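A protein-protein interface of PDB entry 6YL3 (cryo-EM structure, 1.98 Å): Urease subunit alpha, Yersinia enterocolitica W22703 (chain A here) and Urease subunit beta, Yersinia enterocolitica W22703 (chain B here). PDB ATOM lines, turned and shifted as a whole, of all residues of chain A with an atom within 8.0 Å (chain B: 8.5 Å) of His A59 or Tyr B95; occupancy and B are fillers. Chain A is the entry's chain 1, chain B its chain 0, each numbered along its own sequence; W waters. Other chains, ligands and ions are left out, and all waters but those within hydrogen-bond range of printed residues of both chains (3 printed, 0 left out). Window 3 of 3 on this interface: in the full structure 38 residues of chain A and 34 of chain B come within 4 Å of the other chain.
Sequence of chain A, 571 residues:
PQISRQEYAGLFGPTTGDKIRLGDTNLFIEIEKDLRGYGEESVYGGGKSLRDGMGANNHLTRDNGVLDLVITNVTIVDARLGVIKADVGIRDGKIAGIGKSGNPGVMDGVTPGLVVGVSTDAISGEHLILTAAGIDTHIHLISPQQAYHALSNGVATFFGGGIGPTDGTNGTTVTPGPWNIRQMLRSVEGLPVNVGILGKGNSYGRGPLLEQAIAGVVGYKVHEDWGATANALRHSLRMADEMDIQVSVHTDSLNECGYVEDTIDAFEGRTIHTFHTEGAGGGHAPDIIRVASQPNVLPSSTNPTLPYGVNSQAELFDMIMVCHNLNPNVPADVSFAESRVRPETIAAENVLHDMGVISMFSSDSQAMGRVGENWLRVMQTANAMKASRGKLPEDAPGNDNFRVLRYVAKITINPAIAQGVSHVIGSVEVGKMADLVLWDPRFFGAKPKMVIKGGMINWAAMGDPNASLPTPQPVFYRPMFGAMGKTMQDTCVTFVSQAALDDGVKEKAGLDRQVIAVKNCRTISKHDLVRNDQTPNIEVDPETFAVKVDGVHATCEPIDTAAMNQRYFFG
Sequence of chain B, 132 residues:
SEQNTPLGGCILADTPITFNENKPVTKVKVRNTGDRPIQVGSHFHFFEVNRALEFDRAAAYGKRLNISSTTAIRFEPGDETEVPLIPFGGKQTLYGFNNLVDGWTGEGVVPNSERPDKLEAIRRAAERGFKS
O of Gly A105 is in hydrogen-bond range of N of Lys B91 (3.1 Å).
The backbone NH of Thr B93 lies within hydrogen-bond range of the backbone carbonyl oxygen of Gly A105, 3.1 Å away.
The backbone carbonyl oxygen (O) of Tyr B95 is in hydrogen-bond range of the side-chain amide nitrogen (ND2) of Asn A58 (3.4 Å).
The backbone NH (N) of Lys B91 sits at hydrogen-bond distance from the backbone carbonyl oxygen (O) of Pro A104.
O of Gly A105 is in hydrogen-bond range of N of Gln B92 (2.7 Å).
The side-chain amide nitrogen of Asn A103 sits at hydrogen-bond distance from the backbone carbonyl oxygen of Met A54 (2.7 Å).
The backbone carbonyl oxygen of Gln B92 is in hydrogen-bond range of the backbone NH of Thr B105 (2.8 Å).
The indole nitrogen (NE1) of Trp B104 lies close to the backbone carbonyl oxygen (O) of Lys B91 (3.5 Å).
The backbone carbonyl oxygen of Leu B94 lies close to the backbone NH of Asp B102 (3.3 Å).
N of Gly A105 sits close to OD1 of Asn A103 (3.2 Å).
O of Gly B103 is in hydrogen-bond range of N of Leu B94 (2.9 Å).
Gly A53 touches Phe B97.
Phe B97 touches Met A54 (CE2 to CG, 3.2 Å).
Tyr B95 touches His A59.
O of Thr B93 touches CG1 of Val A106, at 3.5 Å.
CD2 of Leu B94 touches CG1 of Val A106, at 3.5 Å.
Printed residues of chain B within 4 Å of Met A54: Phe B97 (3.2 Å).
Asn A58 touches just one residue of chain B: Tyr B95 (3.4 Å).
Of chain B, only Tyr B95 (3.8 Å) comes within 4 Å of His A59.
Printed residues of chain B within 4 Å of Pro A104: Lys B91.
Of the printed residues of chain B, Gly A105 touches Lys B91, Gln B92 and Thr B93.
Of the printed residues of chain B, Val A106 touches Thr B93 and Leu B94.
Of the printed residues of chain A, Leu B94 touches Val A106 (3.5 Å).
Printed residues of chain A within 4 Å of Tyr B95: Asn A58 (3.4 Å) and His A59 (3.8 Å).
Gly B96 touches none of the printed residues of chain A.
Leu B100 touches none of the printed residues of chain A.
The nearest residue of chain B that does not touch His A59 is Thr B93 (5.4 Å).
The nearest printed residue of chain A that does not touch Tyr B95 is Gly A53 (4.01 Å).
Of the 17 printed residues of chain B, 6 touch a printed residue of chain A.
Of the 20 printed residues of chain A, 7 touch a printed residue of chain B.
Hydrophobic or aromatic side chains of chain A that line the printed part of chain B: Met A54, His A59 and Val A106.
Water W2 lies within hydrogen-bond range of O of Gly A53 (2.4 Å), N of Tyr B95 (2.9 Å) and O of Thr B93 (3.3 Å).
Water W1 bridges the side-chain hydroxyl of Thr B93 and a ring nitrogen (NE2) of His A59.
Water W3 bridges OH of Tyr B95 and NE2 of His A59.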
ATOM      1  N   ASP A  52     -10.740  16.868 -34.870  1.00  0.00           N
ATOM      2  CA  ASP A  52     -10.123  17.549 -33.756  1.00  0.00           C
ATOM      3  C   ASP A  52     -10.907  17.337 -32.466  1.00  0.00           C
ATOM      4  O   ASP A  52     -12.075  17.620 -32.431  1.00  0.00           O
ATOM      5  CB  ASP A  52      -9.902  19.050 -33.991  1.00  0.00           C
ATOM      6  CG  ASP A  52     -11.041  19.856 -34.227  1.00  0.00           C
ATOM      7  OD1 ASP A  52     -12.151  19.289 -34.306  1.00  0.00           O
ATOM      8  OD2 ASP A  52     -10.825  21.052 -34.466  1.00  0.00           O
ATOM      9  N   GLY A  53     -10.256  16.830 -31.473  1.00  0.00           N
ATOM     10  CA  GLY A  53     -10.585  16.445 -30.121  1.00  0.00           C
ATOM     11  C   GLY A  53     -11.298  15.150 -29.905  1.00  0.00           C
ATOM     12  O   GLY A  53     -11.621  14.800 -28.817  1.00  0.00           O
ATOM     13  N   MET A  54     -11.589  14.530 -31.021  1.00  0.00           N
ATOM     14  CA  MET A  54     -12.310  13.261 -31.089  1.00  0.00           C
ATOM     15  C   MET A  54     -11.202  12.161 -31.342  1.00  0.00           C
ATOM     16  O   MET A  54     -10.306  12.159 -30.576  1.00  0.00           O
ATOM     17  CB  MET A  54     -13.356  13.444 -32.207  1.00  0.00           C
ATOM     18  CG  MET A  54     -14.435  14.471 -31.916  1.00  0.00           C
ATOM     19  SD  MET A  54     -15.480  15.034 -33.301  1.00  0.00           S
ATOM     20  CE  MET A  54     -15.636  13.568 -34.302  1.00  0.00           C
ATOM     21  N   ALA A  56      -8.559  12.280 -33.234  1.00  0.00           N
ATOM     22  CA  ALA A  56      -7.410  13.123 -33.122  1.00  0.00           C
ATOM     23  C   ALA A  56      -7.301  14.004 -31.896  1.00  0.00           C
ATOM     24  O   ALA A  56      -8.053  14.937 -31.728  1.00  0.00           O
ATOM     25  CB  ALA A  56      -7.252  13.955 -34.374  1.00  0.00           C
ATOM     26  N   ASN A  57      -6.201  13.833 -31.247  1.00  0.00           N
ATOM     27  CA  ASN A  57      -5.634  14.624 -30.272  1.00  0.00           C
ATOM     28  C   ASN A  57      -5.301  15.972 -30.851  1.00  0.00           C
ATOM     29  O   ASN A  57      -4.963  16.082 -32.011  1.00  0.00           O
ATOM     30  CB  ASN A  57      -4.440  13.974 -29.572  1.00  0.00           C
ATOM     31  CG  ASN A  57      -4.015  14.682 -28.443  1.00  0.00           C
ATOM     32  OD1 ASN A  57      -3.421  15.645 -28.531  1.00  0.00           O
ATOM     33  ND2 ASN A  57      -4.430  14.261 -27.371  1.00  0.00           N
ATOM     34  N   ASN A  58      -5.637  16.968 -30.108  1.00  0.00           N
ATOM     35  CA  ASN A  58      -5.589  18.371 -30.428  1.00  0.00           C
ATOM     36  C   ASN A  58      -4.839  19.251 -29.424  1.00  0.00           C
ATOM     37  O   ASN A  58      -4.886  20.409 -29.509  1.00  0.00           O
ATOM     38  CB  ASN A  58      -7.029  18.810 -30.719  1.00  0.00           C
ATOM     39  CG  ASN A  58      -7.908  18.977 -29.486  1.00  0.00           C
ATOM     40  OD1 ASN A  58      -7.642  18.524 -28.460  1.00  0.00           O
ATOM     41  ND2 ASN A  58      -8.995  19.710 -29.694  1.00  0.00           N
ATOM     42  N   HIS A  59      -4.189  18.699 -28.509  1.00  0.00           N
ATOM     43  CA  HIS A  59      -3.488  19.352 -27.479  1.00  0.00           C
ATOM     44  C   HIS A  59      -2.015  19.007 -27.283  1.00  0.00           C
ATOM     45  O   HIS A  59      -1.300  19.806 -26.729  1.00  0.00           O
ATOM     46  CB  HIS A  59      -4.298  19.212 -26.201  1.00  0.00           C
ATOM     47  CG  HIS A  59      -4.208  17.949 -25.449  1.00  0.00           C
ATOM     48  ND1 HIS A  59      -3.368  17.874 -24.432  1.00  0.00           N
ATOM     49  CD2 HIS A  59      -4.885  16.789 -25.459  1.00  0.00           C
ATOM     50  CE1 HIS A  59      -3.433  16.693 -23.886  1.00  0.00           C
ATOM     51  NE2 HIS A  59      -4.379  16.014 -24.466  1.00  0.00           N
ATOM     52  N   LEU A  60      -1.557  17.931 -27.821  1.00  0.00           N
ATOM     53  CA  LEU A  60      -0.221  17.426 -27.791  1.00  0.00           C
ATOM     54  C   LEU A  60       0.618  17.951 -28.966  1.00  0.00           C
ATOM     55  O   LEU A  60       0.164  18.002 -30.097  1.00  0.00           O
ATOM     56  CB  LEU A  60      -0.258  15.903 -27.823  1.00  0.00           C
ATOM     57  CG  LEU A  60      -0.978  15.150 -26.729  1.00  0.00           C
ATOM     58  CD1 LEU A  60      -1.079  13.805 -27.062  1.00  0.00           C
ATOM     59  CD2 LEU A  60      -0.349  15.383 -25.589  1.00  0.00           C
ATOM     60  N   THR A  61       1.771  18.474 -28.626  1.00  0.00           N
ATOM     61  CA  THR A  61       2.860  18.820 -29.512  1.00  0.00           C
ATOM     62  C   THR A  61       3.525  17.529 -29.962  1.00  0.00           C
ATOM     63  O   THR A  61       3.221  16.458 -29.523  1.00  0.00           O
ATOM     64  CB  THR A  61       3.799  19.850 -28.860  1.00  0.00           C
ATOM     65  OG1 THR A  61       4.388  19.332 -27.691  1.00  0.00           O
ATOM     66  CG2 THR A  61       3.184  21.102 -28.800  1.00  0.00           C
ATOM     67  N   ARG A  62       4.309  17.660 -30.958  1.00  0.00           N
ATOM     68  CA  ARG A  62       4.813  16.529 -31.717  1.00  0.00           C
ATOM     69  C   ARG A  62       5.814  15.693 -30.928  1.00  0.00           C
ATOM     70  O   ARG A  62       5.957  14.551 -31.182  1.00  0.00           O
ATOM     71  CB  ARG A  62       5.360  16.981 -33.008  1.00  0.00           C
ATOM     72  CG  ARG A  62       5.653  15.860 -34.032  1.00  0.00           C
ATOM     73  CD  ARG A  62       6.522  16.279 -35.127  1.00  0.00           C
ATOM     74  NE  ARG A  62       7.096  15.232 -35.876  1.00  0.00           N
ATOM     75  CZ  ARG A  62       8.246  14.744 -35.772  1.00  0.00           C
ATOM     76  NH1 ARG A  62       8.531  13.825 -36.559  1.00  0.00           N
ATOM     77  NH2 ARG A  62       9.102  15.323 -35.074  1.00  0.00           N
ATOM     78  N   ASN A  64       5.800  14.791 -27.734  1.00  0.00           N
ATOM     79  CA  ASN A  64       4.987  13.714 -27.202  1.00  0.00           C
ATOM     80  C   ASN A  64       4.771  12.461 -28.010  1.00  0.00           C
ATOM     81  O   ASN A  64       4.103  11.550 -27.608  1.00  0.00           O
ATOM     82  CB  ASN A  64       3.667  14.276 -26.897  1.00  0.00           C
ATOM     83  CG  ASN A  64       3.667  15.323 -25.780  1.00  0.00           C
ATOM     84  OD1 ASN A  64       3.879  16.500 -25.932  1.00  0.00           O
ATOM     85  ND2 ASN A  64       3.208  14.896 -24.761  1.00  0.00           N
ATOM     86  N   VAL A  66       3.527  12.153 -31.112  1.00  0.00           N
ATOM     87  CA  VAL A  66       2.528  12.202 -32.130  1.00  0.00           C
ATOM     88  C   VAL A  66       3.134  11.867 -33.493  1.00  0.00           C
ATOM     89  O   VAL A  66       4.187  12.305 -33.866  1.00  0.00           O
ATOM     90  CB  VAL A  66       1.737  13.527 -32.104  1.00  0.00           C
ATOM     91  CG1 VAL A  66       0.841  13.599 -33.134  1.00  0.00           C
ATOM     92  CG2 VAL A  66       1.174  13.868 -30.776  1.00  0.00           C
ATOM     93  N   ASN A 103      -6.685   8.736 -30.285  1.00  0.00           N
ATOM     94  CA  ASN A 103      -6.665   9.679 -29.218  1.00  0.00           C
ATOM     95  C   ASN A 103      -6.986   9.022 -27.860  1.00  0.00           C
ATOM     96  O   ASN A 103      -8.128   8.742 -27.559  1.00  0.00           O
ATOM     97  CB  ASN A 103      -7.580  10.879 -29.521  1.00  0.00           C
ATOM     98  CG  ASN A 103      -7.579  11.853 -28.518  1.00  0.00           C
ATOM     99  OD1 ASN A 103      -6.750  11.860 -27.682  1.00  0.00           O
ATOM    100  ND2 ASN A 103      -8.443  12.810 -28.664  1.00  0.00           N
ATOM    101  N   PRO A 104      -5.993   8.783 -27.040  1.00  0.00           N
ATOM    102  CA  PRO A 104      -6.186   8.160 -25.748  1.00  0.00           C
ATOM    103  C   PRO A 104      -7.096   8.971 -24.763  1.00  0.00           C
ATOM    104  O   PRO A 104      -7.471   8.475 -23.715  1.00  0.00           O
ATOM    105  CB  PRO A 104      -4.748   8.085 -25.237  1.00  0.00           C
ATOM    106  CG  PRO A 104      -4.038   8.353 -26.215  1.00  0.00           C
ATOM    107  CD  PRO A 104      -4.638   9.224 -27.074  1.00  0.00           C
ATOM    108  N   GLY A 105      -7.325  10.227 -25.039  1.00  0.00           N
ATOM    109  CA  GLY A 105      -8.261  11.010 -24.241  1.00  0.00           C
ATOM    110  C   GLY A 105      -9.688  10.509 -24.233  1.00  0.00           C
ATOM    111  O   GLY A 105     -10.408  10.690 -23.265  1.00  0.00           O
ATOM    112  N   VAL A 106     -10.110   9.977 -25.348  1.00  0.00           N
ATOM    113  CA  VAL A 106     -11.472   9.657 -25.736  1.00  0.00           C
ATOM    114  C   VAL A 106     -11.689   8.235 -26.192  1.00  0.00           C
ATOM    115  O   VAL A 106     -12.791   7.886 -26.489  1.00  0.00           O
ATOM    116  CB  VAL A 106     -12.011  10.685 -26.758  1.00  0.00           C
ATOM    117  CG1 VAL A 106     -11.715  12.147 -26.323  1.00  0.00           C
ATOM    118  CG2 VAL A 106     -11.787  10.411 -28.175  1.00  0.00           C
ATOM    119  N   VAL A 115      -0.493   7.682 -31.418  1.00  0.00           N
ATOM    120  CA  VAL A 115      -1.261   8.883 -31.184  1.00  0.00           C
ATOM    121  C   VAL A 115      -1.296   9.787 -32.393  1.00  0.00           C
ATOM    122  O   VAL A 115      -0.284  10.310 -32.810  1.00  0.00           O
ATOM    123  CB  VAL A 115      -0.891   9.648 -29.917  1.00  0.00           C
ATOM    124  CG1 VAL A 115      -1.786  10.819 -29.885  1.00  0.00           C
ATOM    125  CG2 VAL A 115      -0.843   8.756 -28.695  1.00  0.00           C
ATOM    126  N   VAL A 116      -2.406   9.939 -32.913  1.00  0.00           N
ATOM    127  CA  VAL A 116      -2.799  10.834 -33.962  1.00  0.00           C
ATOM    128  C   VAL A 116      -3.149  12.182 -33.325  1.00  0.00           C
ATOM    129  O   VAL A 116      -3.890  12.276 -32.389  1.00  0.00           O
ATOM    130  CB  VAL A 116      -3.919  10.220 -34.863  1.00  0.00           C
ATOM    131  CG1 VAL A 116      -4.441  11.155 -35.740  1.00  0.00           C
ATOM    132  CG2 VAL A 116      -3.752   8.922 -35.429  1.00  0.00           C
ATOM    133  N   GLY A 117      -2.649  13.216 -33.933  1.00  0.00           N
ATOM    134  CA  GLY A 117      -2.603  14.552 -33.609  1.00  0.00           C
ATOM    135  C   GLY A 117      -2.535  15.596 -34.679  1.00  0.00           C
ATOM    136  O   GLY A 117      -2.589  15.307 -35.825  1.00  0.00           O
ATOM    137  N   VAL A 118      -2.198  16.757 -34.227  1.00  0.00           N
ATOM    138  CA  VAL A 118      -2.078  17.977 -35.034  1.00  0.00           C
ATOM    139  C   VAL A 118      -1.056  17.778 -36.153  1.00  0.00           C
ATOM    140  O   VAL A 118      -1.325  18.110 -37.275  1.00  0.00           O
ATOM    141  CB  VAL A 118      -1.816  19.214 -34.143  1.00  0.00           C
ATOM    142  CG1 VAL A 118      -1.620  20.468 -34.988  1.00  0.00           C
ATOM    143  CG2 VAL A 118      -2.914  19.457 -33.213  1.00  0.00           C
ATOM    144  N   HIS B  45     -19.045  15.099 -29.375  1.00  0.00           N
ATOM    145  CA  HIS B  45     -19.520  15.324 -27.991  1.00  0.00           C
ATOM    146  C   HIS B  45     -20.916  15.897 -28.062  1.00  0.00           C
ATOM    147  O   HIS B  45     -21.078  17.103 -28.155  1.00  0.00           O
ATOM    148  CB  HIS B  45     -18.696  16.205 -27.106  1.00  0.00           C
ATOM    149  CG  HIS B  45     -19.135  16.224 -25.697  1.00  0.00           C
ATOM    150  ND1 HIS B  45     -18.744  17.156 -24.830  1.00  0.00           N
ATOM    151  CD2 HIS B  45     -19.908  15.390 -24.986  1.00  0.00           C
ATOM    152  CE1 HIS B  45     -19.254  16.914 -23.676  1.00  0.00           C
ATOM    153  NE2 HIS B  45     -19.938  15.829 -23.735  1.00  0.00           N
ATOM    154  N   GLU B  48     -22.508  19.297 -27.021  1.00  0.00           N
ATOM    155  CA  GLU B  48     -21.989  20.466 -27.642  1.00  0.00           C
ATOM    156  C   GLU B  48     -22.456  20.626 -29.057  1.00  0.00           C
ATOM    157  O   GLU B  48     -22.063  21.572 -29.698  1.00  0.00           O
ATOM    158  CB  GLU B  48     -20.463  20.533 -27.444  1.00  0.00           C
ATOM    159  CG  GLU B  48     -19.790  20.199 -26.287  1.00  0.00           C
ATOM    160  CD  GLU B  48     -18.416  20.875 -25.981  1.00  0.00           C
ATOM    161  OE1 GLU B  48     -18.140  21.996 -26.327  1.00  0.00           O
ATOM    162  OE2 GLU B  48     -17.620  20.231 -25.393  1.00  0.00           O
ATOM    163  N   LYS B  91      -9.455   8.430 -21.299  1.00  0.00           N
ATOM    164  CA  LYS B  91      -9.375   9.304 -20.160  1.00  0.00           C
ATOM    165  C   LYS B  91     -10.630  10.215 -19.982  1.00  0.00           C
ATOM    166  O   LYS B  91     -10.729  10.853 -18.976  1.00  0.00           O
ATOM    167  CB  LYS B  91      -8.053  10.102 -20.100  1.00  0.00           C
ATOM    168  CG  LYS B  91      -6.789   9.205 -19.651  1.00  0.00           C
ATOM    169  CD  LYS B  91      -5.562   9.742 -19.455  1.00  0.00           C
ATOM    170  CE  LYS B  91      -4.942  10.114 -20.813  1.00  0.00           C
ATOM    171  NZ  LYS B  91      -4.376  11.308 -20.491  1.00  0.00           N
ATOM    172  N   GLN B  92     -11.597  10.222 -20.859  1.00  0.00           N
ATOM    173  CA  GLN B  92     -12.782  11.069 -20.788  1.00  0.00           C
ATOM    174  C   GLN B  92     -12.472  12.533 -20.647  1.00  0.00           C
ATOM    175  O   GLN B  92     -13.109  13.257 -19.928  1.00  0.00           O
ATOM    176  CB  GLN B  92     -13.741  10.508 -19.702  1.00  0.00           C
ATOM    177  CG  GLN B  92     -14.370   9.399 -20.112  1.00  0.00           C
ATOM    178  CD  GLN B  92     -15.134   8.501 -19.151  1.00  0.00           C
ATOM    179  OE1 GLN B  92     -14.739   8.299 -18.055  1.00  0.00           O
ATOM    180  NE2 GLN B  92     -16.095   7.836 -19.663  1.00  0.00           N
ATOM    181  N   THR B  93     -11.519  12.965 -21.398  1.00  0.00           N
ATOM    182  CA  THR B  93     -10.994  14.288 -21.553  1.00  0.00           C
ATOM    183  C   THR B  93     -11.330  14.820 -22.949  1.00  0.00           C
ATOM    184  O   THR B  93     -10.743  14.439 -23.923  1.00  0.00           O
ATOM    185  CB  THR B  93      -9.519  14.409 -21.192  1.00  0.00           C
ATOM    186  OG1 THR B  93      -8.644  13.683 -22.057  1.00  0.00           O
ATOM    187  CG2 THR B  93      -9.276  13.982 -19.762  1.00  0.00           C
ATOM    188  N   LEU B  94     -12.147  15.794 -22.952  1.00  0.00           N
ATOM    189  CA  LEU B  94     -12.761  16.443 -24.053  1.00  0.00           C
ATOM    190  C   LEU B  94     -12.343  17.909 -24.120  1.00  0.00           C
ATOM    191  O   LEU B  94     -12.736  18.740 -23.315  1.00  0.00           O
ATOM    192  CB  LEU B  94     -14.232  16.190 -24.047  1.00  0.00           C
ATOM    193  CG  LEU B  94     -14.830  14.794 -24.206  1.00  0.00           C
ATOM    194  CD1 LEU B  94     -16.310  14.920 -24.176  1.00  0.00           C
ATOM    195  CD2 LEU B  94     -14.510  14.102 -25.400  1.00  0.00           C
ATOM    196  N   TYR B  95     -11.459  18.216 -25.085  1.00  0.00           N
ATOM    197  CA  TYR B  95     -10.959  19.583 -25.340  1.00  0.00           C
ATOM    198  C   TYR B  95     -11.513  20.099 -26.661  1.00  0.00           C
ATOM    199  O   TYR B  95     -11.588  19.347 -27.536  1.00  0.00           O
ATOM    200  CB  TYR B  95      -9.443  19.631 -25.222  1.00  0.00           C
ATOM    201  CG  TYR B  95      -8.837  19.048 -23.963  1.00  0.00           C
ATOM    202  CD1 TYR B  95      -8.876  19.765 -22.792  1.00  0.00           C
ATOM    203  CD2 TYR B  95      -8.186  17.827 -23.955  1.00  0.00           C
ATOM    204  CE1 TYR B  95      -8.299  19.317 -21.628  1.00  0.00           C
ATOM    205  CE2 TYR B  95      -7.575  17.344 -22.797  1.00  0.00           C
ATOM    206  CZ  TYR B  95      -7.636  18.100 -21.635  1.00  0.00           C
ATOM    207  OH  TYR B  95      -7.066  17.661 -20.490  1.00  0.00           O
ATOM    208  N   GLY B  96     -11.819  21.375 -26.779  1.00  0.00           N
ATOM    209  CA  GLY B  96     -12.341  21.950 -28.018  1.00  0.00           C
ATOM    210  C   GLY B  96     -13.843  21.807 -28.202  1.00  0.00           C
ATOM    211  O   GLY B  96     -14.495  22.242 -27.346  1.00  0.00           O
ATOM    212  N   PHE B  97     -14.337  21.423 -29.381  1.00  0.00           N
ATOM    213  CA  PHE B  97     -15.777  21.401 -29.762  1.00  0.00           C
ATOM    214  C   PHE B  97     -16.256  22.888 -29.612  1.00  0.00           C
ATOM    215  O   PHE B  97     -15.664  23.727 -30.269  1.00  0.00           O
ATOM    216  CB  PHE B  97     -16.565  20.270 -29.029  1.00  0.00           C
ATOM    217  CG  PHE B  97     -16.006  18.873 -29.085  1.00  0.00           C
ATOM    218  CD1 PHE B  97     -15.087  18.456 -28.141  1.00  0.00           C
ATOM    219  CD2 PHE B  97     -16.394  18.003 -30.076  1.00  0.00           C
ATOM    220  CE1 PHE B  97     -14.563  17.179 -28.210  1.00  0.00           C
ATOM    221  CE2 PHE B  97     -15.860  16.733 -30.152  1.00  0.00           C
ATOM    222  CZ  PHE B  97     -14.969  16.329 -29.199  1.00  0.00           C
ATOM    223  N   ASN B  98     -17.163  23.256 -28.713  1.00  0.00           N
ATOM    224  CA  ASN B  98     -17.744  24.609 -28.540  1.00  0.00           C
ATOM    225  C   ASN B  98     -17.255  25.318 -27.286  1.00  0.00           C
ATOM    226  O   ASN B  98     -17.746  26.344 -26.899  1.00  0.00           O
ATOM    227  CB  ASN B  98     -19.236  24.620 -28.662  1.00  0.00           C
ATOM    228  CG  ASN B  98     -19.740  24.784 -30.049  1.00  0.00           C
ATOM    229  OD1 ASN B  98     -19.378  25.630 -30.770  1.00  0.00           O
ATOM    230  ND2 ASN B  98     -20.574  24.001 -30.374  1.00  0.00           N
ATOM    231  N   ASN B  99     -16.280  24.780 -26.690  1.00  0.00           N
ATOM    232  CA  ASN B  99     -15.577  25.204 -25.533  1.00  0.00           C
ATOM    233  C   ASN B  99     -16.475  25.241 -24.281  1.00  0.00           C
ATOM    234  O   ASN B  99     -16.278  26.011 -23.381  1.00  0.00           O
ATOM    235  CB  ASN B  99     -14.753  26.456 -25.805  1.00  0.00           C
ATOM    236  CG  ASN B  99     -13.757  26.275 -26.981  1.00  0.00           C
ATOM    237  OD1 ASN B  99     -13.933  26.808 -28.003  1.00  0.00           O
ATOM    238  ND2 ASN B  99     -12.758  25.473 -26.772  1.00  0.00           N
ATOM    239  N   LEU B 100     -17.386  24.281 -24.210  1.00  0.00           N
ATOM    240  CA  LEU B 100     -18.306  24.024 -23.105  1.00  0.00           C
ATOM    241  C   LEU B 100     -17.724  23.280 -21.901  1.00  0.00           C
ATOM    242  O   LEU B 100     -18.138  23.520 -20.785  1.00  0.00           O
ATOM    243  CB  LEU B 100     -19.530  23.325 -23.602  1.00  0.00           C
ATOM    244  CG  LEU B 100     -20.525  24.147 -24.448  1.00  0.00           C
ATOM    245  CD1 LEU B 100     -21.660  23.566 -24.801  1.00  0.00           C
ATOM    246  CD2 LEU B 100     -20.762  25.503 -24.091  1.00  0.00           C
ATOM    247  N   VAL B 101     -16.857  22.347 -22.104  1.00  0.00           N
ATOM    248  CA  VAL B 101     -16.169  21.532 -21.121  1.00  0.00           C
ATOM    249  C   VAL B 101     -14.677  21.831 -21.021  1.00  0.00           C
ATOM    250  O   VAL B 101     -14.220  22.333 -19.992  1.00  0.00           O
ATOM    251  CB  VAL B 101     -16.516  20.065 -21.307  1.00  0.00           C
ATOM    252  CG1 VAL B 101     -15.913  19.277 -20.231  1.00  0.00           C
ATOM    253  CG2 VAL B 101     -18.062  19.874 -21.384  1.00  0.00           C
ATOM    254  N   ASP B 102     -13.909  21.549 -22.053  1.00  0.00           N
ATOM    255  CA  ASP B 102     -12.476  21.678 -21.996  1.00  0.00           C
ATOM    256  C   ASP B 102     -11.868  21.063 -20.731  1.00  0.00           C
ATOM    257  O   ASP B 102     -11.186  21.698 -19.951  1.00  0.00           O
ATOM    258  CB  ASP B 102     -12.069  23.130 -22.233  1.00  0.00           C
ATOM    259  CG  ASP B 102     -12.438  23.648 -23.627  1.00  0.00           C
ATOM    260  OD1 ASP B 102     -12.324  22.891 -24.564  1.00  0.00           O
ATOM    261  OD2 ASP B 102     -12.834  24.826 -23.704  1.00  0.00           O
ATOM    262  N   GLY B 103     -12.257  19.853 -20.532  1.00  0.00           N
ATOM    263  CA  GLY B 103     -11.900  18.902 -19.595  1.00  0.00           C
ATOM    264  C   GLY B 103     -12.474  17.514 -19.442  1.00  0.00           C
ATOM    265  O   GLY B 103     -12.914  16.868 -20.355  1.00  0.00           O
ATOM    266  N   TRP B 104     -12.440  17.095 -18.224  1.00  0.00           N
ATOM    267  CA  TRP B 104     -12.805  15.789 -17.768  1.00  0.00           C
ATOM    268  C   TRP B 104     -14.299  15.699 -17.649  1.00  0.00           C
ATOM    269  O   TRP B 104     -14.916  16.537 -17.062  1.00  0.00           O
ATOM    270  CB  TRP B 104     -12.218  15.294 -16.478  1.00  0.00           C
ATOM    271  CG  TRP B 104     -12.358  14.144 -16.136  1.00  0.00           C
ATOM    272  CD1 TRP B 104     -12.137  13.120 -16.800  1.00  0.00           C
ATOM    273  CD2 TRP B 104     -12.736  13.693 -14.861  1.00  0.00           C
ATOM    274  NE1 TRP B 104     -12.379  12.048 -16.137  1.00  0.00           N
ATOM    275  CE2 TRP B 104     -12.774  12.390 -14.906  1.00  0.00           C
ATOM    276  CE3 TRP B 104     -13.067  14.279 -13.692  1.00  0.00           C
ATOM    277  CZ2 TRP B 104     -13.046  11.695 -13.816  1.00  0.00           C
ATOM    278  CZ3 TRP B 104     -13.347  13.562 -12.728  1.00  0.00           C
ATOM    279  CH2 TRP B 104     -13.346  12.382 -12.766  1.00  0.00           C
ATOM    280  N   THR B 105     -14.817  14.699 -18.206  1.00  0.00           N
ATOM    281  CA  THR B 105     -16.220  14.374 -18.298  1.00  0.00           C
ATOM    282  C   THR B 105     -16.624  13.097 -17.610  1.00  0.00           C
ATOM    283  O   THR B 105     -17.721  12.667 -17.763  1.00  0.00           O
ATOM    284  CB  THR B 105     -16.638  14.518 -19.771  1.00  0.00           C
ATOM    285  OG1 THR B 105     -15.894  13.690 -20.524  1.00  0.00           O
ATOM    286  CG2 THR B 105     -16.527  15.804 -20.236  1.00  0.00           C
HETATM  287  O   HOH W   1      -7.592  14.834 -24.492  1.00  0.00           O
HETATM  288  O   HOH W   2     -10.925  15.983 -26.805  1.00  0.00           O
HETATM  289  O   HOH W   3      -4.879  15.687 -21.358  1.00  0.00           O
